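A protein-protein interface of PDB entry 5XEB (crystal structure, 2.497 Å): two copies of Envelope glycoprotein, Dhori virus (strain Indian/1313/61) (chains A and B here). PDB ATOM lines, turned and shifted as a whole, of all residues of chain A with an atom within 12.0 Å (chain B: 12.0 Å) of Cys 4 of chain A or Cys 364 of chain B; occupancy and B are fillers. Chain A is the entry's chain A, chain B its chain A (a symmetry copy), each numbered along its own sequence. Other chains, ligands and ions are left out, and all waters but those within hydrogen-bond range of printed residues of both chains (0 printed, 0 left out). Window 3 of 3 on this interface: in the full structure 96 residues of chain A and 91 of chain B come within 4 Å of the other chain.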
ATOM      1  N   CYS A   4      20.573   2.296  -9.958  1.00  0.00           N
ATOM      2  CA  CYS A   4      19.495   1.478 -10.499  1.00  0.00           C
ATOM      3  C   CYS A   4      19.723   1.184 -11.980  1.00  0.00           C
ATOM      4  O   CYS A   4      20.472   0.272 -12.334  1.00  0.00           O
ATOM      5  CB  CYS A   4      18.145   2.173 -10.299  1.00  0.00           C
ATOM      6  SG  CYS A   4      16.725   1.257 -10.940  1.00  0.00           S
ATOM      7  N   ASN A   5      19.048   1.966 -12.825  1.00  0.00           N
ATOM      8  CA  ASN A   5      19.168   1.947 -14.282  1.00  0.00           C
ATOM      9  C   ASN A   5      18.545   0.696 -14.888  1.00  0.00           C
ATOM     10  O   ASN A   5      18.216  -0.256 -14.175  1.00  0.00           O
ATOM     11  CB  ASN A   5      20.631   2.100 -14.703  1.00  0.00           C
ATOM     12  CG  ASN A   5      21.211   3.438 -14.292  1.00  0.00           C
ATOM     13  OD1 ASN A   5      21.076   4.433 -15.006  1.00  0.00           O
ATOM     14  ND2 ASN A   5      21.846   3.475 -13.127  1.00  0.00           N
ATOM     15  N   LYS A   6      18.373   0.699 -16.208  1.00  0.00           N
ATOM     16  CA  LYS A   6      17.559  -0.283 -16.907  1.00  0.00           C
ATOM     17  C   LYS A   6      18.358  -0.932 -18.029  1.00  0.00           C
ATOM     18  O   LYS A   6      19.418  -0.449 -18.434  1.00  0.00           O
ATOM     19  CB  LYS A   6      16.294   0.369 -17.485  1.00  0.00           C
ATOM     20  CG  LYS A   6      15.027   0.110 -16.695  1.00  0.00           C
ATOM     21  CD  LYS A   6      14.533  -1.308 -16.912  1.00  0.00           C
ATOM     22  CE  LYS A   6      14.250  -1.568 -18.383  1.00  0.00           C
ATOM     23  NZ  LYS A   6      13.794  -2.962 -18.630  1.00  0.00           N
ATOM     24  N   ALA A   7      17.833  -2.057 -18.524  1.00  0.00           N
ATOM     25  CA  ALA A   7      18.251  -2.596 -19.811  1.00  0.00           C
ATOM     26  C   ALA A   7      17.611  -1.848 -20.970  1.00  0.00           C
ATOM     27  O   ALA A   7      18.032  -2.028 -22.119  1.00  0.00           O
ATOM     28  CB  ALA A   7      17.910  -4.087 -19.902  1.00  0.00           C
ATOM     29  N   GLN A   8      16.589  -1.044 -20.686  1.00  0.00           N
ATOM     30  CA  GLN A   8      16.088  -0.056 -21.629  1.00  0.00           C
ATOM     31  C   GLN A   8      17.235   0.761 -22.208  1.00  0.00           C
ATOM     32  O   GLN A   8      18.148   1.178 -21.488  1.00  0.00           O
ATOM     33  CB  GLN A   8      15.091   0.859 -20.911  1.00  0.00           C
ATOM     34  CG  GLN A   8      15.037   2.285 -21.419  1.00  0.00           C
ATOM     35  CD  GLN A   8      14.268   2.399 -22.710  1.00  0.00           C
ATOM     36  OE1 GLN A   8      14.771   2.052 -23.777  1.00  0.00           O
ATOM     37  NE2 GLN A   8      13.032   2.875 -22.622  1.00  0.00           N
ATOM     38  N   GLN A   9      17.193   0.982 -23.521  1.00  0.00           N
ATOM     39  CA  GLN A   9      18.177   1.817 -24.205  1.00  0.00           C
ATOM     40  C   GLN A   9      17.449   2.803 -25.125  1.00  0.00           C
ATOM     41  O   GLN A   9      17.618   2.815 -26.343  1.00  0.00           O
ATOM     42  CB  GLN A   9      19.202   0.959 -24.956  1.00  0.00           C
ATOM     43  CG  GLN A   9      18.642  -0.001 -26.002  1.00  0.00           C
ATOM     44  CD  GLN A   9      19.741  -0.685 -26.797  1.00  0.00           C
ATOM     45  OE1 GLN A   9      20.826  -0.945 -26.277  1.00  0.00           O
ATOM     46  NE2 GLN A   9      19.468  -0.969 -28.066  1.00  0.00           N
ATOM     47  N   GLN A  10      16.618   3.655 -24.517  1.00  0.00           N
ATOM     48  CA  GLN A  10      15.839   4.637 -25.269  1.00  0.00           C
ATOM     49  C   GLN A  10      16.793   5.678 -25.849  1.00  0.00           C
ATOM     50  O   GLN A  10      17.038   6.744 -25.279  1.00  0.00           O
ATOM     51  CB  GLN A  10      14.775   5.291 -24.398  1.00  0.00           C
ATOM     52  CG  GLN A  10      13.847   6.205 -25.183  1.00  0.00           C
ATOM     53  CD  GLN A  10      12.969   7.059 -24.295  1.00  0.00           C
ATOM     54  OE1 GLN A  10      12.837   6.802 -23.099  1.00  0.00           O
ATOM     55  NE2 GLN A  10      12.364   8.089 -24.878  1.00  0.00           N
ATOM     56  N   ASP B 338      29.375   7.661 -17.359  1.00  0.00           N
ATOM     57  CA  ASP B 338      28.079   7.484 -18.001  1.00  0.00           C
ATOM     58  C   ASP B 338      26.971   8.296 -17.345  1.00  0.00           C
ATOM     59  O   ASP B 338      25.880   8.396 -17.918  1.00  0.00           O
ATOM     60  CB  ASP B 338      27.698   6.000 -18.024  1.00  0.00           C
ATOM     61  CG  ASP B 338      27.546   5.410 -16.635  1.00  0.00           C
ATOM     62  OD1 ASP B 338      28.040   6.020 -15.664  1.00  0.00           O
ATOM     63  OD2 ASP B 338      26.938   4.326 -16.518  1.00  0.00           O
ATOM     64  N   ARG B 339      27.214   8.874 -16.170  1.00  0.00           N
ATOM     65  CA  ARG B 339      26.269   9.789 -15.544  1.00  0.00           C
ATOM     66  C   ARG B 339      26.503  11.241 -15.948  1.00  0.00           C
ATOM     67  O   ARG B 339      25.793  12.127 -15.460  1.00  0.00           O
ATOM     68  CB  ARG B 339      26.337   9.661 -14.016  1.00  0.00           C
ATOM     69  CG  ARG B 339      26.134   8.244 -13.496  1.00  0.00           C
ATOM     70  CD  ARG B 339      24.699   7.756 -13.680  1.00  0.00           C
ATOM     71  NE  ARG B 339      23.795   8.259 -12.646  1.00  0.00           N
ATOM     72  CZ  ARG B 339      22.824   9.142 -12.859  1.00  0.00           C
ATOM     73  NH1 ARG B 339      22.615   9.624 -14.077  1.00  0.00           N
ATOM     74  NH2 ARG B 339      22.056   9.539 -11.854  1.00  0.00           N
ATOM     75  N   LEU B 340      27.472  11.500 -16.829  1.00  0.00           N
ATOM     76  CA  LEU B 340      27.814  12.868 -17.209  1.00  0.00           C
ATOM     77  C   LEU B 340      26.678  13.526 -17.986  1.00  0.00           C
ATOM     78  O   LEU B 340      26.141  14.560 -17.572  1.00  0.00           O
ATOM     79  CB  LEU B 340      29.109  12.860 -18.029  1.00  0.00           C
ATOM     80  CG  LEU B 340      29.741  14.155 -18.560  1.00  0.00           C
ATOM     81  CD1 LEU B 340      29.147  14.590 -19.897  1.00  0.00           C
ATOM     82  CD2 LEU B 340      29.655  15.271 -17.534  1.00  0.00           C
ATOM     83  N   LEU B 341      26.306  12.934 -19.127  1.00  0.00           N
ATOM     84  CA  LEU B 341      25.266  13.508 -19.975  1.00  0.00           C
ATOM     85  C   LEU B 341      23.965  13.725 -19.212  1.00  0.00           C
ATOM     86  O   LEU B 341      23.214  14.658 -19.520  1.00  0.00           O
ATOM     87  CB  LEU B 341      25.026  12.604 -21.184  1.00  0.00           C
ATOM     88  CG  LEU B 341      26.139  12.587 -22.233  1.00  0.00           C
ATOM     89  CD1 LEU B 341      26.007  11.382 -23.149  1.00  0.00           C
ATOM     90  CD2 LEU B 341      26.110  13.873 -23.040  1.00  0.00           C
ATOM     91  N   GLY B 342      23.685  12.881 -18.218  1.00  0.00           N
ATOM     92  CA  GLY B 342      22.499  13.033 -17.404  1.00  0.00           C
ATOM     93  C   GLY B 342      22.463  14.351 -16.664  1.00  0.00           C
ATOM     94  O   GLY B 342      21.519  15.133 -16.809  1.00  0.00           O
ATOM     95  N   THR B 343      23.495  14.612 -15.858  1.00  0.00           N
ATOM     96  CA  THR B 343      23.567  15.876 -15.139  1.00  0.00           C
ATOM     97  C   THR B 343      23.722  17.043 -16.102  1.00  0.00           C
ATOM     98  O   THR B 343      23.343  18.172 -15.770  1.00  0.00           O
ATOM     99  CB  THR B 343      24.724  15.852 -14.143  1.00  0.00           C
ATOM    100  OG1 THR B 343      25.968  15.883 -14.850  1.00  0.00           O
ATOM    101  CG2 THR B 343      24.668  14.585 -13.294  1.00  0.00           C
ATOM    102  N   GLY B 346      20.211  17.833 -16.966  1.00  0.00           N
ATOM    103  CA  GLY B 346      19.293  17.838 -15.842  1.00  0.00           C
ATOM    104  C   GLY B 346      18.367  16.627 -15.762  1.00  0.00           C
ATOM    105  O   GLY B 346      17.467  16.610 -14.913  1.00  0.00           O
ATOM    106  N   GLN B 347      18.572  15.621 -16.613  1.00  0.00           N
ATOM    107  CA  GLN B 347      17.749  14.422 -16.702  1.00  0.00           C
ATOM    108  C   GLN B 347      18.467  13.287 -15.994  1.00  0.00           C
ATOM    109  O   GLN B 347      19.693  13.176 -16.071  1.00  0.00           O
ATOM    110  CB  GLN B 347      17.499  14.049 -18.163  1.00  0.00           C
ATOM    111  CG  GLN B 347      16.789  15.126 -18.960  1.00  0.00           C
ATOM    112  CD  GLN B 347      16.534  14.682 -20.377  1.00  0.00           C
ATOM    113  OE1 GLN B 347      16.678  13.502 -20.696  1.00  0.00           O
ATOM    114  NE2 GLN B 347      16.162  15.618 -21.240  1.00  0.00           N
ATOM    115  N   ASP B 348      17.707  12.474 -15.289  1.00  0.00           N
ATOM    116  CA  ASP B 348      18.264  11.338 -14.578  1.00  0.00           C
ATOM    117  C   ASP B 348      18.433  10.205 -15.577  1.00  0.00           C
ATOM    118  O   ASP B 348      17.458   9.567 -15.983  1.00  0.00           O
ATOM    119  CB  ASP B 348      17.342  10.966 -13.434  1.00  0.00           C
ATOM    120  CG  ASP B 348      17.962   9.997 -12.513  1.00  0.00           C
ATOM    121  OD1 ASP B 348      19.196   9.815 -12.560  1.00  0.00           O
ATOM    122  OD2 ASP B 348      17.198   9.424 -11.737  1.00  0.00           O
ATOM    123  N   VAL B 349      19.678   9.954 -15.981  1.00  0.00           N
ATOM    124  CA  VAL B 349      19.933   9.134 -17.157  1.00  0.00           C
ATOM    125  C   VAL B 349      21.411   8.751 -17.220  1.00  0.00           C
ATOM    126  O   VAL B 349      22.284   9.511 -16.785  1.00  0.00           O
ATOM    127  CB  VAL B 349      19.466   9.886 -18.423  1.00  0.00           C
ATOM    128  CG1 VAL B 349      20.604  10.654 -19.073  1.00  0.00           C
ATOM    129  CG2 VAL B 349      18.785   8.958 -19.410  1.00  0.00           C
ATOM    130  N   SER B 350      21.684   7.550 -17.723  1.00  0.00           N
ATOM    131  CA  SER B 350      23.007   7.004 -17.974  1.00  0.00           C
ATOM    132  C   SER B 350      23.110   6.650 -19.450  1.00  0.00           C
ATOM    133  O   SER B 350      22.113   6.292 -20.089  1.00  0.00           O
ATOM    134  CB  SER B 350      23.268   5.755 -17.123  1.00  0.00           C
ATOM    135  OG  SER B 350      24.171   4.874 -17.772  1.00  0.00           O
ATOM    136  N   SER B 351      24.324   6.747 -19.987  1.00  0.00           N
ATOM    137  CA  SER B 351      24.560   6.578 -21.410  1.00  0.00           C
ATOM    138  C   SER B 351      25.463   5.379 -21.668  1.00  0.00           C
ATOM    139  O   SER B 351      26.247   4.971 -20.806  1.00  0.00           O
ATOM    140  CB  SER B 351      25.198   7.833 -22.017  1.00  0.00           C
ATOM    141  OG  SER B 351      26.548   7.959 -21.605  1.00  0.00           O
ATOM    142  N   LYS B 352      25.334   4.818 -22.868  1.00  0.00           N
ATOM    143  CA  LYS B 352      26.235   3.783 -23.362  1.00  0.00           C
ATOM    144  C   LYS B 352      26.507   4.071 -24.828  1.00  0.00           C
ATOM    145  O   LYS B 352      25.571   4.132 -25.632  1.00  0.00           O
ATOM    146  CB  LYS B 352      25.642   2.382 -23.189  1.00  0.00           C
ATOM    147  CG  LYS B 352      26.087   1.665 -21.925  1.00  0.00           C
ATOM    148  CD  LYS B 352      26.252   0.175 -22.186  1.00  0.00           C
ATOM    149  CE  LYS B 352      25.344  -0.656 -21.297  1.00  0.00           C
ATOM    150  NZ  LYS B 352      25.771  -0.630 -19.870  1.00  0.00           N
ATOM    151  N   MET B 360      23.240   5.747 -26.188  1.00  0.00           N
ATOM    152  CA  MET B 360      21.915   5.328 -25.749  1.00  0.00           C
ATOM    153  C   MET B 360      21.730   5.665 -24.271  1.00  0.00           C
ATOM    154  O   MET B 360      22.703   5.815 -23.528  1.00  0.00           O
ATOM    155  CB  MET B 360      21.703   3.822 -25.982  1.00  0.00           C
ATOM    156  CG  MET B 360      20.571   3.493 -26.946  1.00  0.00           C
ATOM    157  SD  MET B 360      21.053   3.358 -28.677  1.00  0.00           S
ATOM    158  CE  MET B 360      21.588   1.651 -28.760  1.00  0.00           C
ATOM    159  N   LEU B 361      20.468   5.769 -23.838  1.00  0.00           N
ATOM    160  CA  LEU B 361      20.132   6.360 -22.543  1.00  0.00           C
ATOM    161  C   LEU B 361      19.164   5.486 -21.741  1.00  0.00           C
ATOM    162  O   LEU B 361      18.322   4.783 -22.311  1.00  0.00           O
ATOM    163  CB  LEU B 361      19.526   7.761 -22.739  1.00  0.00           C
ATOM    164  CG  LEU B 361      20.433   8.966 -22.461  1.00  0.00           C
ATOM    165  CD1 LEU B 361      21.779   8.826 -23.129  1.00  0.00           C
ATOM    166  CD2 LEU B 361      19.758  10.271 -22.865  1.00  0.00           C
ATOM    167  N   SER B 362      19.285   5.556 -20.412  1.00  0.00           N
ATOM    168  CA  SER B 362      18.477   4.801 -19.458  1.00  0.00           C
ATOM    169  C   SER B 362      18.340   5.626 -18.182  1.00  0.00           C
ATOM    170  O   SER B 362      19.197   6.459 -17.891  1.00  0.00           O
ATOM    171  CB  SER B 362      19.116   3.439 -19.154  1.00  0.00           C
ATOM    172  OG  SER B 362      19.561   2.821 -20.347  1.00  0.00           O
ATOM    173  N   PRO B 363      17.282   5.408 -17.381  1.00  0.00           N
ATOM    174  CA  PRO B 363      16.940   6.417 -16.360  1.00  0.00           C
ATOM    175  C   PRO B 363      17.316   6.093 -14.915  1.00  0.00           C
ATOM    176  O   PRO B 363      18.498   5.952 -14.581  1.00  0.00           O
ATOM    177  CB  PRO B 363      15.419   6.523 -16.508  1.00  0.00           C
ATOM    178  CG  PRO B 363      14.989   5.154 -17.057  1.00  0.00           C
ATOM    179  CD  PRO B 363      16.227   4.390 -17.479  1.00  0.00           C
ATOM    180  N   CYS B 364      16.294   6.072 -14.044  1.00  0.00           N
ATOM    181  CA  CYS B 364      16.328   5.591 -12.661  1.00  0.00           C
ATOM    182  C   CYS B 364      16.950   6.544 -11.643  1.00  0.00           C
ATOM    183  O   CYS B 364      18.120   6.921 -11.768  1.00  0.00           O
ATOM    184  CB  CYS B 364      17.064   4.256 -12.575  1.00  0.00           C
ATOM    185  SG  CYS B 364      16.070   2.860 -12.004  1.00  0.00           S
ATOM    186  N   LEU B 365      16.169   6.915 -10.625  1.00  0.00           N
ATOM    187  CA  LEU B 365      16.685   7.500  -9.382  1.00  0.00           C
ATOM    188  C   LEU B 365      16.355   6.565  -8.225  1.00  0.00           C
ATOM    189  O   LEU B 365      17.079   6.502  -7.234  1.00  0.00           O
ATOM    190  CB  LEU B 365      16.090   8.891  -9.115  1.00  0.00           C
ATOM    191  CG  LEU B 365      16.963   9.951  -8.420  1.00  0.00           C
ATOM    192  CD1 LEU B 365      16.878   9.865  -6.901  1.00  0.00           C
ATOM    193  CD2 LEU B 365      18.419   9.900  -8.883  1.00  0.00           C
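Of chain B, only Cys 364 comes within 4 Å of Cys 4 of chain A.
Of chain A, only Cys 4 and Asn 5 come within 4 Å of Cys 364 of chain B.
No residue of chain A comes within 4 Å of Asp 348 of chain B.
Pro 363 of chain B touches one residue of chain A.
Leu 365 of chain B touches none of the printed residues of chain A.
Of the printed residues of chain B, Asn 5 of chain A touches Ser 350, Ser 362, Pro 363 and Cys 364.
Of the printed residues of chain A, Ser 362 of chain B touches Asn 5 (3.99 Å), Lys 6 (3.8 Å) and Gln 8 (2.4 Å).
Of the printed residues of chain B, Gln 8 of chain A touches Leu 361 and Ser 362.
Printed residues of chain A within 4 Å of Met 360 of chain B: Gln 9.
Gly 346 of chain B touches none of the printed residues of chain A.
Gln 347 of chain B touches none of the printed residues of chain A.
The nearest residue of chain A that does not touch Cys 364 of chain B is Lys 6 of chain A (5.3 Å).
O of Gln 8 of chain A lies within hydrogen-bond range of OG of Ser 362 of chain B (2.4 Å).
The backbone carbonyl oxygen of Pro 363 of chain B lies close to the side-chain amide oxygen of Asn 5 of chain A.
N of Gln 10 of chain A is in hydrogen-bond range of O of Leu 361 of chain B (3.0 Å).
SG of Cys 4 of chain A is disulfide-bonded to SG of Cys 364 of chain B (2.0 Å).
N of Asn 5 of chain A lies close to SG of Cys 364 of chain B, 3.2 Å away.
Of the 7 printed residues of chain A, 6 touch a printed residue of chain B.
Printed residues of chain A that touch a printed residue of chain B: Cys 4, Asn 5, Lys 6, Gln 8, Gln 9 and Gln 10.
Hydrophobic or aromatic side chains of chain B that line the printed part of chain A: Met 360 and Leu 361.
Among the printed residues, 11 pairs touch across the chains.
No position is printed for both chains.
Of the 11 pairs that touch across the chains among the printed residues, none has its exchanged pair printed and touching as well.
Among the printed residues, merely in contact across the chains: Gln 9 of chain A with Met 360 of chain B (3.1 Å), Asn 5 of chain A with Ser 350 of chain B (3.3 Å), Gln 9 of chain A with Leu 361 of chain B (3.5 Å), Gln 8 of chain A with Leu 361 of chain B (3.7 Å), Lys 6 of chain A with Ser 362 of chain B (3.8 Å) and Asn 5 of chain A with Ser 362 of chain B (3.99 Å).
The side-chain carboxylate (OD2) of Asp 348 of chain B sits close to the backbone carbonyl oxygen (O) of Cys 364 of chain B, 2.7 Å away.
The backbone NH of Ser 350 of chain B lies within hydrogen-bond range of the backbone carbonyl oxygen of Ser 362 of chain B (2.7 Å).
OE1 of Gln 8 of chain A lies within hydrogen-bond range of N of Gln 10 of chain A, 2.6 Å away.
OD2 of Asp 338 of chain B sits at hydrogen-bond distance from OG of Ser 350 of chain B (3.1 Å).
The backbone NH (N) of Lys 352 of chain B is in hydrogen-bond range of the backbone carbonyl oxygen (O) of Met 360 of chain B.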
